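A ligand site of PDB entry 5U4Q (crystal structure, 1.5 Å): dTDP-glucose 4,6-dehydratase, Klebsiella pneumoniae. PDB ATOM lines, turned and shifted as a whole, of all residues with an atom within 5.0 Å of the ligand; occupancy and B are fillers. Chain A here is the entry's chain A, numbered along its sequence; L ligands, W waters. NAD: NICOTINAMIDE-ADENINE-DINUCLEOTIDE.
OD1 of Asp 63 sits at hydrogen-bond distance from N6A of the ligand.
The backbone NH (N) of Val 184 is in hydrogen-bond range of an oxygen (O7N) of the ligand (2.8 Å).
The backbone NH (N) of Asn 35 sits at hydrogen-bond distance from a nitrogen (N3A) of the ligand (3.1 Å).
NH1 of Arg 190 is in salt-bridge range of O2N of the ligand, at 3.0 Å.
The backbone NH (N) of Ile 15 lies within hydrogen-bond range of an oxygen (O1N) of the ligand (2.8 Å).
The side-chain hydroxyl (OH) of Tyr 154 sits at hydrogen-bond distance from an oxygen (O2D) of the ligand, 2.6 Å away.
The side-chain amino group of Lys 158 sits at hydrogen-bond distance from an oxygen (O3D) of the ligand.
An oxygen (O1A) of the ligand sits at hydrogen-bond distance from the side-chain hydroxyl (OH) of Tyr 40 (2.5 Å).
An oxygen (O2B) of the ligand sits close to the side-chain amide nitrogen (ND2) of Asn 37.
N of Leu 64 sits at hydrogen-bond distance from N1A of the ligand, at 3.0 Å.
An oxygen (O3B) of the ligand sits at hydrogen-bond distance from the backbone NH (N) of Gly 13 (3.2 Å).
An oxygen (O2B) of the ligand lies within hydrogen-bond range of the side-chain carboxylate (OD1) of Asp 34 (2.5 Å).
The side-chain amide oxygen (OD1) of Asn 35 sits close to an oxygen (O2B) of the ligand (3.4 Å).
N of Phe 14 sits at hydrogen-bond distance from O1A of the ligand, at 3.0 Å.
The backbone carbonyl oxygen (O) of Leu 85 is in hydrogen-bond range of an oxygen (O3D) of the ligand, at 2.8 Å.
An oxygen (O2B) of the ligand sits at hydrogen-bond distance from the side-chain amino group (NZ) of Lys 45.
NH1 of Arg 190 sits close to SD of Met 193, 3.5 Å away.
The backbone carbonyl oxygen (O) of Ala 89 lies within hydrogen-bond range of the guanidinium group (NH2) of Arg 190 (2.7 Å).
N of Gly 13 sits at hydrogen-bond distance from OD2 of Asp 34 (3.5 Å).
The side-chain amino group (NZ) of Lys 158 lies within hydrogen-bond range of the backbone carbonyl oxygen (O) of Ala 127 (3.0 Å).
The side-chain carboxylate of Asp 63 lies within hydrogen-bond range of the side-chain amide nitrogen of Asn 35 (3.0 Å).
The side-chain carboxylate of Asp 63 lies within hydrogen-bond range of the backbone NH of Ala 65, at 3.1 Å.
The side-chain carboxylate (OD1) of Asp 34 is in hydrogen-bond range of the backbone NH (N) of Met 36.
The backbone carbonyl oxygen (O) of Asn 37 sits at hydrogen-bond distance from the side-chain amino group (NZ) of Lys 45, at 2.8 Å.
Merely in contact with the ligand: Phe 182 (3.0 Å), Leu 62 (3.3 Å), Phe 181 (3.3 Å), Ala 87 (3.3 Å), Ala 127 (3.4 Å), Ala 86 (3.4 Å), Thr 183 (3.5 Å), Ala 89 (3.5 Å), Gly 10 (3.6 Å), Ala 104 (3.6 Å), Ala 12 (3.7 Å), Ser 128 (3.8 Å) and Met 36 (3.9 Å).
Within 4 Å of the ligand: Gly 10, Ala 12, Gly 13, Phe 14, Ile 15, Asp 34, Asn 35, Met 36, Asn 37, Tyr 40, Lys 45, Leu 62, Asp 63, Leu 64, Leu 85, Ala 86, Ala 87, Ala 89, Ala 104, Ala 127, Ser 128, Tyr 154, Lys 158, Phe 181, Phe 182, Thr 183, Val 184 and Arg 190.
Along chain A the residues within 4 Å of the ligand span positions 10 to 190.
The nearest printed residue that does not touch the ligand is Met 193 (4.2 Å).
Water W4 bridges OG of Ser 129 (2.6 Å) and OH of Tyr 154 (2.7 Å).
Water W1 lies within hydrogen-bond range of O1N of the ligand (2.8 Å), N of Gly 16 (2.9 Å) and O of Gly 10 (2.9 Å).
Water W7 bridges NZ of Lys 45 (2.8 Å) and O2A of the ligand (2.8 Å).
Water W6 lies within hydrogen-bond range of the backbone carbonyl oxygen (O) of Ala 86, an oxygen (O3D) of the ligand, the side-chain amino group (NZ) of Lys 158 and the backbone carbonyl oxygen (O) of Leu 85.
Water W2 lies within hydrogen-bond range of O of Val 184 and N7N of the ligand.
Water W3 bridges the side-chain amide nitrogen (ND2) of Asn 37 (2.9 Å) and the backbone carbonyl oxygen (O) of Ala 87 (3.5 Å).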
ATOM      1  N   GLY A  10      16.958 -24.604 -14.762  1.00  0.00           N
ATOM      2  CA  GLY A  10      17.415 -23.872 -13.579  1.00  0.00           C
ATOM      3  C   GLY A  10      16.235 -23.203 -12.908  1.00  0.00           C
ATOM      4  O   GLY A  10      16.393 -22.192 -12.217  1.00  0.00           O
ATOM      5  N   ALA A  12      14.443 -23.813 -10.306  1.00  0.00           N
ATOM      6  CA  ALA A  12      14.438 -23.676  -8.834  1.00  0.00           C
ATOM      7  C   ALA A  12      15.483 -22.681  -8.370  1.00  0.00           C
ATOM      8  O   ALA A  12      15.561 -22.391  -7.166  1.00  0.00           O
ATOM      9  CB  ALA A  12      14.677 -25.006  -8.153  1.00  0.00           C
ATOM     10  N   GLY A  13      16.281 -22.165  -9.317  1.00  0.00           N
ATOM     11  CA  GLY A  13      17.287 -21.162  -9.024  1.00  0.00           C
ATOM     12  C   GLY A  13      16.722 -19.770  -9.072  1.00  0.00           C
ATOM     13  O   GLY A  13      15.573 -19.565  -9.353  1.00  0.00           O
ATOM     14  N   PHE A  14      17.568 -18.793  -8.781  1.00  0.00           N
ATOM     15  CA  PHE A  14      17.162 -17.397  -8.698  1.00  0.00           C
ATOM     16  C   PHE A  14      16.505 -16.843  -9.932  1.00  0.00           C
ATOM     17  O   PHE A  14      15.328 -16.497  -9.927  1.00  0.00           O
ATOM     18  CB  PHE A  14      18.400 -16.561  -8.306  1.00  0.00           C
ATOM     19  CG  PHE A  14      18.201 -15.062  -8.277  1.00  0.00           C
ATOM     20  CD1 PHE A  14      17.016 -14.462  -7.927  1.00  0.00           C
ATOM     21  CD2 PHE A  14      19.311 -14.233  -8.502  1.00  0.00           C
ATOM     22  CE1 PHE A  14      16.901 -13.075  -7.867  1.00  0.00           C
ATOM     23  CE2 PHE A  14      19.206 -12.865  -8.441  1.00  0.00           C
ATOM     24  CZ  PHE A  14      18.006 -12.284  -8.131  1.00  0.00           C
ATOM     25  N   ILE A  15      17.261 -16.752 -11.014  1.00  0.00           N
ATOM     26  CA  ILE A  15      16.739 -16.139 -12.215  1.00  0.00           C
ATOM     27  C   ILE A  15      15.633 -17.018 -12.831  1.00  0.00           C
ATOM     28  O   ILE A  15      14.585 -16.513 -13.199  1.00  0.00           O
ATOM     29  CB  ILE A  15      17.857 -15.802 -13.218  1.00  0.00           C
ATOM     30  CG1 ILE A  15      18.856 -14.861 -12.542  1.00  0.00           C
ATOM     31  CG2 ILE A  15      17.282 -15.162 -14.471  1.00  0.00           C
ATOM     32  CD1 ILE A  15      20.023 -14.493 -13.417  1.00  0.00           C
ATOM     33  N   GLY A  16      15.875 -18.336 -12.923  1.00  0.00           N
ATOM     34  CA  GLY A  16      14.882 -19.248 -13.512  1.00  0.00           C
ATOM     35  C   GLY A  16      13.552 -19.236 -12.823  1.00  0.00           C
ATOM     36  O   GLY A  16      12.497 -19.268 -13.487  1.00  0.00           O
ATOM     37  N   ASP A  34      15.446 -28.747 -12.832  1.00  0.00           N
ATOM     38  CA  ASP A  34      16.541 -28.366 -11.983  1.00  0.00           C
ATOM     39  C   ASP A  34      17.024 -29.652 -11.339  1.00  0.00           C
ATOM     40  O   ASP A  34      16.222 -30.541 -11.116  1.00  0.00           O
ATOM     41  CB  ASP A  34      16.029 -27.380 -10.936  1.00  0.00           C
ATOM     42  CG  ASP A  34      17.119 -26.540 -10.330  1.00  0.00           C
ATOM     43  OD1 ASP A  34      17.993 -27.105  -9.613  1.00  0.00           O
ATOM     44  OD2 ASP A  34      17.099 -25.306 -10.577  1.00  0.00           O
ATOM     45  N   ASN A  35      18.307 -29.738 -11.032  1.00  0.00           N
ATOM     46  CA  ASN A  35      18.799 -30.923 -10.325  1.00  0.00           C
ATOM     47  C   ASN A  35      18.837 -30.768  -8.819  1.00  0.00           C
ATOM     48  O   ASN A  35      19.285 -31.690  -8.121  1.00  0.00           O
ATOM     49  CB  ASN A  35      20.148 -31.384 -10.895  1.00  0.00           C
ATOM     50  CG  ASN A  35      21.306 -30.479 -10.534  1.00  0.00           C
ATOM     51  OD1 ASN A  35      21.143 -29.406  -9.947  1.00  0.00           O
ATOM     52  ND2 ASN A  35      22.517 -30.920 -10.878  1.00  0.00           N
ATOM     53  N   MET A  36      18.401 -29.605  -8.321  1.00  0.00           N
ATOM     54  CA  MET A  36      18.322 -29.340  -6.870  1.00  0.00           C
ATOM     55  C   MET A  36      19.645 -29.574  -6.212  1.00  0.00           C
ATOM     56  O   MET A  36      19.715 -30.117  -5.112  1.00  0.00           O
ATOM     57  CB  MET A  36      17.219 -30.212  -6.221  1.00  0.00           C
ATOM     58  CG  MET A  36      15.881 -30.108  -6.954  1.00  0.00           C
ATOM     59  SD  MET A  36      15.184 -28.261  -6.995  1.00  0.00           S
ATOM     60  CE  MET A  36      14.567 -28.090  -5.147  1.00  0.00           C
ATOM     61  N   ASN A  37      20.730 -29.147  -6.850  1.00  0.00           N
ATOM     62  CA  ASN A  37      22.055 -29.391  -6.256  1.00  0.00           C
ATOM     63  C   ASN A  37      22.253 -28.548  -5.011  1.00  0.00           C
ATOM     64  O   ASN A  37      21.560 -27.551  -4.795  1.00  0.00           O
ATOM     65  CB  ASN A  37      23.204 -29.225  -7.256  1.00  0.00           C
ATOM     66  CG  ASN A  37      23.478 -27.769  -7.623  1.00  0.00           C
ATOM     67  OD1 ASN A  37      23.631 -26.922  -6.752  1.00  0.00           O
ATOM     68  ND2 ASN A  37      23.560 -27.482  -8.912  1.00  0.00           N
ATOM     69  N   TYR A  40      24.172 -24.222  -2.886  1.00  0.00           N
ATOM     70  CA  TYR A  40      23.691 -23.380  -1.777  1.00  0.00           C
ATOM     71  C   TYR A  40      22.424 -24.068  -1.290  1.00  0.00           C
ATOM     72  O   TYR A  40      21.965 -25.021  -1.925  1.00  0.00           O
ATOM     73  CB  TYR A  40      23.497 -21.886  -2.130  1.00  0.00           C
ATOM     74  CG  TYR A  40      22.478 -21.546  -3.198  1.00  0.00           C
ATOM     75  CD1 TYR A  40      21.117 -21.574  -2.912  1.00  0.00           C
ATOM     76  CD2 TYR A  40      22.874 -21.176  -4.467  1.00  0.00           C
ATOM     77  CE1 TYR A  40      20.173 -21.245  -3.873  1.00  0.00           C
ATOM     78  CE2 TYR A  40      21.937 -20.858  -5.438  1.00  0.00           C
ATOM     79  CZ  TYR A  40      20.583 -20.887  -5.136  1.00  0.00           C
ATOM     80  OH  TYR A  40      19.649 -20.553  -6.113  1.00  0.00           O
ATOM     81  N   LYS A  45      15.892 -23.372  -2.745  1.00  0.00           N
ATOM     82  CA  LYS A  45      15.443 -23.837  -4.062  1.00  0.00           C
ATOM     83  C   LYS A  45      14.038 -24.447  -3.974  1.00  0.00           C
ATOM     84  O   LYS A  45      13.190 -24.178  -4.816  1.00  0.00           O
ATOM     85  CB  LYS A  45      16.448 -24.819  -4.661  1.00  0.00           C
ATOM     86  CG  LYS A  45      17.790 -24.175  -4.977  1.00  0.00           C
ATOM     87  CD  LYS A  45      18.787 -25.171  -5.549  1.00  0.00           C
ATOM     88  CE  LYS A  45      20.099 -24.466  -5.828  1.00  0.00           C
ATOM     89  NZ  LYS A  45      21.122 -25.339  -6.444  1.00  0.00           N
ATOM     90  N   ARG A  48      11.453 -21.750  -3.677  1.00  0.00           N
ATOM     91  CA  ARG A  48      11.109 -21.118  -4.941  1.00  0.00           C
ATOM     92  C   ARG A  48      10.158 -22.007  -5.730  1.00  0.00           C
ATOM     93  O   ARG A  48       9.174 -21.534  -6.264  1.00  0.00           O
ATOM     94  CB  ARG A  48      12.357 -20.853  -5.758  1.00  0.00           C
ATOM     95  CG  ARG A  48      13.321 -19.860  -5.126  1.00  0.00           C
ATOM     96  CD  ARG A  48      14.320 -19.379  -6.174  1.00  0.00           C
ATOM     97  NE  ARG A  48      15.510 -18.705  -5.629  1.00  0.00           N
ATOM     98  CZ  ARG A  48      16.679 -19.285  -5.353  1.00  0.00           C
ATOM     99  NH1 ARG A  48      16.886 -20.583  -5.560  1.00  0.00           N
ATOM    100  NH2 ARG A  48      17.698 -18.558  -4.891  1.00  0.00           N
ATOM    101  N   LEU A  62      15.856 -33.130 -12.929  1.00  0.00           N
ATOM    102  CA  LEU A  62      16.608 -33.688 -14.032  1.00  0.00           C
ATOM    103  C   LEU A  62      17.929 -32.986 -14.121  1.00  0.00           C
ATOM    104  O   LEU A  62      17.994 -31.750 -13.940  1.00  0.00           O
ATOM    105  CB  LEU A  62      15.819 -33.438 -15.323  1.00  0.00           C
ATOM    106  CG  LEU A  62      16.314 -33.931 -16.648  1.00  0.00           C
ATOM    107  CD1 LEU A  62      16.436 -35.434 -16.666  1.00  0.00           C
ATOM    108  CD2 LEU A  62      15.347 -33.475 -17.732  1.00  0.00           C
ATOM    109  N   ASP A  63      18.977 -33.744 -14.400  1.00  0.00           N
ATOM    110  CA  ASP A  63      20.289 -33.198 -14.606  1.00  0.00           C
ATOM    111  C   ASP A  63      20.506 -32.917 -16.081  1.00  0.00           C
ATOM    112  O   ASP A  63      20.168 -33.723 -16.949  1.00  0.00           O
ATOM    113  CB  ASP A  63      21.362 -34.153 -14.102  1.00  0.00           C
ATOM    114  CG  ASP A  63      22.635 -33.435 -13.748  1.00  0.00           C
ATOM    115  OD1 ASP A  63      23.273 -32.885 -14.666  1.00  0.00           O
ATOM    116  OD2 ASP A  63      22.951 -33.406 -12.531  1.00  0.00           O
ATOM    117  N   LEU A  64      21.067 -31.756 -16.389  1.00  0.00           N
ATOM    118  CA  LEU A  64      21.375 -31.367 -17.783  1.00  0.00           C
ATOM    119  C   LEU A  64      22.276 -32.389 -18.488  1.00  0.00           C
ATOM    120  O   LEU A  64      22.193 -32.521 -19.720  1.00  0.00           O
ATOM    121  CB  LEU A  64      22.095 -30.025 -17.807  1.00  0.00           C
ATOM    122  CG  LEU A  64      21.356 -28.771 -17.394  1.00  0.00           C
ATOM    123  CD1 LEU A  64      22.375 -27.643 -17.387  1.00  0.00           C
ATOM    124  CD2 LEU A  64      20.190 -28.484 -18.340  1.00  0.00           C
ATOM    125  N   ALA A  65      23.099 -33.100 -17.714  1.00  0.00           N
ATOM    126  CA  ALA A  65      24.041 -34.062 -18.249  1.00  0.00           C
ATOM    127  C   ALA A  65      23.457 -35.441 -18.481  1.00  0.00           C
ATOM    128  O   ALA A  65      24.149 -36.310 -19.015  1.00  0.00           O
ATOM    129  CB  ALA A  65      25.220 -34.162 -17.310  1.00  0.00           C
ATOM    130  N   LEU A  85      18.922 -21.488 -18.286  1.00  0.00           N
ATOM    131  CA  LEU A  85      19.589 -20.777 -17.194  1.00  0.00           C
ATOM    132  C   LEU A  85      20.403 -21.695 -16.292  1.00  0.00           C
ATOM    133  O   LEU A  85      21.306 -21.248 -15.586  1.00  0.00           O
ATOM    134  CB  LEU A  85      18.563 -19.997 -16.387  1.00  0.00           C
ATOM    135  CG  LEU A  85      17.786 -18.943 -17.185  1.00  0.00           C
ATOM    136  CD1 LEU A  85      16.524 -18.500 -16.453  1.00  0.00           C
ATOM    137  CD2 LEU A  85      18.658 -17.751 -17.552  1.00  0.00           C
ATOM    138  N   ALA A  86      20.129 -22.997 -16.297  1.00  0.00           N
ATOM    139  CA  ALA A  86      20.844 -23.947 -15.458  1.00  0.00           C
ATOM    140  C   ALA A  86      22.321 -23.998 -15.828  1.00  0.00           C
ATOM    141  O   ALA A  86      22.665 -24.138 -17.005  1.00  0.00           O
ATOM    142  CB  ALA A  86      20.240 -25.339 -15.559  1.00  0.00           C
ATOM    143  N   ALA A  87      23.165 -23.875 -14.805  1.00  0.00           N
ATOM    144  CA  ALA A  87      24.617 -23.910 -14.964  1.00  0.00           C
ATOM    145  C   ALA A  87      25.272 -23.886 -13.601  1.00  0.00           C
ATOM    146  O   ALA A  87      24.651 -23.508 -12.604  1.00  0.00           O
ATOM    147  CB  ALA A  87      25.128 -22.729 -15.780  1.00  0.00           C
ATOM    148  N   GLN A  88      26.540 -24.277 -13.621  1.00  0.00           N
ATOM    149  CA  GLN A  88      27.436 -24.201 -12.516  1.00  0.00           C
ATOM    150  C   GLN A  88      28.034 -22.817 -12.631  1.00  0.00           C
ATOM    151  O   GLN A  88      28.618 -22.492 -13.667  1.00  0.00           O
ATOM    152  CB  GLN A  88      28.545 -25.242 -12.695  1.00  0.00           C
ATOM    153  CG  GLN A  88      29.567 -25.288 -11.583  1.00  0.00           C
ATOM    154  CD  GLN A  88      29.011 -25.850 -10.293  1.00  0.00           C
ATOM    155  OE1 GLN A  88      28.097 -26.690 -10.314  1.00  0.00           O
ATOM    156  NE2 GLN A  88      29.578 -25.419  -9.182  1.00  0.00           N
ATOM    157  N   ALA A  89      27.869 -21.997 -11.606  1.00  0.00           N
ATOM    158  CA  ALA A  89      28.362 -20.614 -11.630  1.00  0.00           C
ATOM    159  C   ALA A  89      28.700 -20.204 -10.218  1.00  0.00           C
ATOM    160  O   ALA A  89      27.827 -20.258  -9.361  1.00  0.00           O
ATOM    161  CB  ALA A  89      27.289 -19.691 -12.206  1.00  0.00           C
ATOM    162  N   ALA A 104      27.800 -29.577 -16.425  1.00  0.00           N
ATOM    163  CA  ALA A 104      26.622 -28.752 -16.557  1.00  0.00           C
ATOM    164  C   ALA A 104      26.729 -27.794 -17.720  1.00  0.00           C
ATOM    165  O   ALA A 104      25.728 -27.549 -18.435  1.00  0.00           O
ATOM    166  CB  ALA A 104      26.400 -27.957 -15.293  1.00  0.00           C
ATOM    167  N   ALA A 127      21.774 -18.277 -21.037  1.00  0.00           N
ATOM    168  CA  ALA A 127      22.620 -17.416 -20.214  1.00  0.00           C
ATOM    169  C   ALA A 127      24.084 -17.543 -20.580  1.00  0.00           C
ATOM    170  O   ALA A 127      24.657 -18.637 -20.558  1.00  0.00           O
ATOM    171  CB  ALA A 127      22.426 -17.785 -18.751  1.00  0.00           C
ATOM    172  N   SER A 128      24.689 -16.426 -20.922  1.00  0.00           N
ATOM    173  CA  SER A 128      26.129 -16.290 -21.023  1.00  0.00           C
ATOM    174  C   SER A 128      26.562 -15.444 -19.808  1.00  0.00           C
ATOM    175  O   SER A 128      25.864 -15.426 -18.777  1.00  0.00           O
ATOM    176  CB  SER A 128      26.552 -15.691 -22.350  1.00  0.00           C
ATOM    177  OG  SER A 128      27.977 -15.678 -22.476  1.00  0.00           O
ATOM    178  N   SER A 129      27.716 -14.790 -19.899  1.00  0.00           N
ATOM    179  CA  SER A 129      28.226 -14.062 -18.756  1.00  0.00           C
ATOM    180  C   SER A 129      29.203 -12.973 -19.161  1.00  0.00           C
ATOM    181  O   SER A 129      29.960 -13.155 -20.105  1.00  0.00           O
ATOM    182  CB  SER A 129      28.984 -15.044 -17.850  1.00  0.00           C
ATOM    183  OG  SER A 129      29.788 -14.371 -16.878  1.00  0.00           O
ATOM    184  N   TYR A 154      34.793 -21.055 -15.869  1.00  0.00           N
ATOM    185  CA  TYR A 154      33.400 -20.611 -16.013  1.00  0.00           C
ATOM    186  C   TYR A 154      33.255 -19.747 -17.272  1.00  0.00           C
ATOM    187  O   TYR A 154      32.410 -20.023 -18.135  1.00  0.00           O
ATOM    188  CB  TYR A 154      32.956 -19.853 -14.758  1.00  0.00           C
ATOM    189  CG  TYR A 154      31.610 -19.184 -14.875  1.00  0.00           C
ATOM    190  CD1 TYR A 154      30.438 -19.924 -14.935  1.00  0.00           C
ATOM    191  CD2 TYR A 154      31.522 -17.814 -14.889  1.00  0.00           C
ATOM    192  CE1 TYR A 154      29.198 -19.306 -15.011  1.00  0.00           C
ATOM    193  CE2 TYR A 154      30.294 -17.174 -14.950  1.00  0.00           C
ATOM    194  CZ  TYR A 154      29.131 -17.926 -15.020  1.00  0.00           C
ATOM    195  OH  TYR A 154      27.914 -17.281 -15.097  1.00  0.00           O
ATOM    196  N   LYS A 158      31.195 -20.439 -20.901  1.00  0.00           N
ATOM    197  CA  LYS A 158      30.157 -19.567 -21.433  1.00  0.00           C
ATOM    198  C   LYS A 158      30.447 -19.153 -22.868  1.00  0.00           C
ATOM    199  O   LYS A 158      29.529 -19.114 -23.729  1.00  0.00           O
ATOM    200  CB  LYS A 158      29.880 -18.389 -20.493  1.00  0.00           C
ATOM    201  CG  LYS A 158      29.255 -18.784 -19.148  1.00  0.00           C
ATOM    202  CD  LYS A 158      27.943 -19.567 -19.300  1.00  0.00           C
ATOM    203  CE  LYS A 158      27.097 -19.505 -18.031  1.00  0.00           C
ATOM    204  NZ  LYS A 158      25.738 -20.177 -18.204  1.00  0.00           N
ATOM    205  N   PHE A 181      25.071 -11.807 -18.835  1.00  0.00           N
ATOM    206  CA  PHE A 181      24.658 -11.253 -17.549  1.00  0.00           C
ATOM    207  C   PHE A 181      25.871 -10.708 -16.782  1.00  0.00           C
ATOM    208  O   PHE A 181      26.976 -11.223 -16.874  1.00  0.00           O
ATOM    209  CB  PHE A 181      24.001 -12.331 -16.697  1.00  0.00           C
ATOM    210  CG  PHE A 181      22.614 -12.738 -17.165  1.00  0.00           C
ATOM    211  CD1 PHE A 181      21.489 -11.983 -16.838  1.00  0.00           C
ATOM    212  CD2 PHE A 181      22.429 -13.876 -17.925  1.00  0.00           C
ATOM    213  CE1 PHE A 181      20.223 -12.373 -17.258  1.00  0.00           C
ATOM    214  CE2 PHE A 181      21.176 -14.273 -18.326  1.00  0.00           C
ATOM    215  CZ  PHE A 181      20.062 -13.513 -18.016  1.00  0.00           C
ATOM    216  N   PHE A 182      25.624  -9.649 -16.008  1.00  0.00           N
ATOM    217  CA  PHE A 182      26.618  -9.042 -15.143  1.00  0.00           C
ATOM    218  C   PHE A 182      26.277  -9.497 -13.704  1.00  0.00           C
ATOM    219  O   PHE A 182      26.554 -10.654 -13.377  1.00  0.00           O
ATOM    220  CB  PHE A 182      26.637  -7.518 -15.409  1.00  0.00           C
ATOM    221  CG  PHE A 182      27.357  -7.179 -16.696  1.00  0.00           C
ATOM    222  CD1 PHE A 182      26.813  -7.525 -17.927  1.00  0.00           C
ATOM    223  CD2 PHE A 182      28.636  -6.610 -16.657  1.00  0.00           C
ATOM    224  CE1 PHE A 182      27.503  -7.264 -19.098  1.00  0.00           C
ATOM    225  CE2 PHE A 182      29.326  -6.344 -17.815  1.00  0.00           C
ATOM    226  CZ  PHE A 182      28.769  -6.687 -19.041  1.00  0.00           C
ATOM    227  N   THR A 183      25.701  -8.664 -12.870  1.00  0.00           N
ATOM    228  CA  THR A 183      25.218  -9.118 -11.562  1.00  0.00           C
ATOM    229  C   THR A 183      23.729  -8.772 -11.428  1.00  0.00           C
ATOM    230  O   THR A 183      23.305  -7.669 -11.745  1.00  0.00           O
ATOM    231  CB  THR A 183      26.039  -8.464 -10.462  1.00  0.00           C
ATOM    232  OG1 THR A 183      27.402  -8.864 -10.607  1.00  0.00           O
ATOM    233  CG2 THR A 183      25.544  -8.862  -9.069  1.00  0.00           C
ATOM    234  N   VAL A 184      22.965  -9.747 -10.960  1.00  0.00           N
ATOM    235  CA  VAL A 184      21.523  -9.586 -10.756  1.00  0.00           C
ATOM    236  C   VAL A 184      21.265  -9.676  -9.248  1.00  0.00           C
ATOM    237  O   VAL A 184      21.942 -10.397  -8.547  1.00  0.00           O
ATOM    238  CB  VAL A 184      20.742 -10.670 -11.531  1.00  0.00           C
ATOM    239  CG1 VAL A 184      19.246 -10.452 -11.381  1.00  0.00           C
ATOM    240  CG2 VAL A 184      21.164 -10.656 -12.992  1.00  0.00           C
ATOM    241  N   ARG A 190      20.457 -15.325  -4.694  1.00  0.00           N
ATOM    242  CA  ARG A 190      21.336 -16.395  -4.267  1.00  0.00           C
ATOM    243  C   ARG A 190      22.253 -15.942  -3.117  1.00  0.00           C
ATOM    244  O   ARG A 190      22.800 -14.818  -3.149  1.00  0.00           O
ATOM    245  CB  ARG A 190      22.079 -17.000  -5.451  1.00  0.00           C
ATOM    246  CG  ARG A 190      22.642 -15.981  -6.371  1.00  0.00           C
ATOM    247  CD  ARG A 190      23.045 -16.600  -7.671  1.00  0.00           C
ATOM    248  NE  ARG A 190      24.169 -17.502  -7.500  1.00  0.00           N
ATOM    249  CZ  ARG A 190      24.921 -17.943  -8.517  1.00  0.00           C
ATOM    250  NH1 ARG A 190      24.678 -17.570  -9.770  1.00  0.00           N
ATOM    251  NH2 ARG A 190      25.937 -18.752  -8.252  1.00  0.00           N
ATOM    252  N   MET A 193      25.928 -14.279  -3.613  1.00  0.00           N
ATOM    253  CA  MET A 193      26.143 -13.119  -4.457  1.00  0.00           C
ATOM    254  C   MET A 193      25.341 -11.908  -4.085  1.00  0.00           C
ATOM    255  O   MET A 193      24.340 -12.000  -3.374  1.00  0.00           O
ATOM    256  CB  MET A 193      25.727 -13.444  -5.905  1.00  0.00           C
ATOM    257  CG  MET A 193      26.410 -14.689  -6.439  1.00  0.00           C
ATOM    258  SD  MET A 193      26.302 -14.808  -8.401  1.00  0.00           S
ATOM    259  CE  MET A 193      27.783 -16.078  -8.630  1.00  0.00           C
HETATM  260  PA  NAD L   1      21.280 -20.273  -9.405  1.00  0.00           P
HETATM  261  O1A NAD L   1      20.389 -19.672  -8.381  1.00  0.00           O
HETATM  262  O2A NAD L   1      22.451 -21.136  -8.981  1.00  0.00           O
HETATM  263  O5B NAD L   1      20.345 -21.080 -10.443  1.00  0.00           O
HETATM  264  C5B NAD L   1      20.829 -22.066 -11.348  1.00  0.00           C
HETATM  265  C4B NAD L   1      20.024 -23.337 -11.122  1.00  0.00           C
HETATM  266  O4B NAD L   1      20.599 -24.303 -12.036  1.00  0.00           O
HETATM  267  C3B NAD L   1      20.142 -23.896  -9.712  1.00  0.00           C
HETATM  268  O3B NAD L   1      18.897 -23.981  -8.997  1.00  0.00           O
HETATM  269  C2B NAD L   1      20.811 -25.256  -9.933  1.00  0.00           C
HETATM  270  O2B NAD L   1      20.319 -26.275  -9.053  1.00  0.00           O
HETATM  271  C1B NAD L   1      20.562 -25.563 -11.414  1.00  0.00           C
HETATM  272  N9A NAD L   1      21.577 -26.449 -12.003  1.00  0.00           N
HETATM  273  C8A NAD L   1      22.927 -26.300 -11.949  1.00  0.00           C
HETATM  274  N7A NAD L   1      23.530 -27.311 -12.573  1.00  0.00           N
HETATM  275  C5A NAD L   1      22.556 -28.111 -13.065  1.00  0.00           C
HETATM  276  C6A NAD L   1      22.535 -29.385 -13.810  1.00  0.00           C
HETATM  277  N6A NAD L   1      23.648 -30.002 -14.188  1.00  0.00           N
HETATM  278  N1A NAD L   1      21.328 -29.882 -14.089  1.00  0.00           N
HETATM  279  C2A NAD L   1      20.187 -29.300 -13.716  1.00  0.00           C
HETATM  280  N3A NAD L   1      20.128 -28.152 -13.013  1.00  0.00           N
HETATM  281  C4A NAD L   1      21.300 -27.541 -12.673  1.00  0.00           C
HETATM  282  O3  NAD L   1      21.956 -19.147 -10.341  1.00  0.00           O
HETATM  283  PN  NAD L   1      21.253 -17.945 -11.143  1.00  0.00           P
HETATM  284  O1N NAD L   1      19.791 -18.035 -11.165  1.00  0.00           O
HETATM  285  O2N NAD L   1      21.998 -16.701 -10.662  1.00  0.00           O
HETATM  286  O5D NAD L   1      21.834 -18.267 -12.592  1.00  0.00           O
HETATM  287  C5D NAD L   1      21.063 -18.486 -13.772  1.00  0.00           C
HETATM  288  C4D NAD L   1      22.026 -18.372 -14.946  1.00  0.00           C
HETATM  289  O4D NAD L   1      22.438 -16.998 -15.100  1.00  0.00           O
HETATM  290  C3D NAD L   1      23.313 -19.183 -14.887  1.00  0.00           C
HETATM  291  O3D NAD L   1      23.559 -19.701 -16.197  1.00  0.00           O
HETATM  292  C2D NAD L   1      24.388 -18.170 -14.571  1.00  0.00           C
HETATM  293  O2D NAD L   1      25.685 -18.521 -15.115  1.00  0.00           O
HETATM  294  C1D NAD L   1      23.856 -16.903 -15.204  1.00  0.00           C
HETATM  295  N1N NAD L   1      24.314 -15.689 -14.513  1.00  0.00           N
HETATM  296  C2N NAD L   1      23.749 -15.231 -13.369  1.00  0.00           C
HETATM  297  C3N NAD L   1      24.216 -14.063 -12.736  1.00  0.00           C
HETATM  298  C7N NAD L   1      23.631 -13.481 -11.442  1.00  0.00           C
HETATM  299  O7N NAD L   1      24.000 -12.363 -11.061  1.00  0.00           O
HETATM  300  N7N NAD L   1      22.764 -14.151 -10.662  1.00  0.00           N
HETATM  301  C4N NAD L   1      25.285 -13.392 -13.283  1.00  0.00           C
HETATM  302  C5N NAD L   1      25.862 -13.880 -14.454  1.00  0.00           C
HETATM  303  C6N NAD L   1      25.383 -15.043 -15.044  1.00  0.00           C
HETATM  304  O   HOH W   1      18.206 -19.913 -12.469  1.00  0.00           O
HETATM  305  O   HOH W   2      22.714 -12.940  -7.834  1.00  0.00           O
HETATM  306  O   HOH W   3      24.685 -24.861  -9.396  1.00  0.00           O
HETATM  307  O   HOH W   4      28.476 -14.701 -14.715  1.00  0.00           O
HETATM  308  O   HOH W   5      28.776 -12.145 -14.598  1.00  0.00           O
HETATM  309  O   HOH W   6      22.890 -21.567 -18.490  1.00  0.00           O
HETATM  310  O   HOH W   7      23.015 -23.498  -7.496  1.00  0.00           O
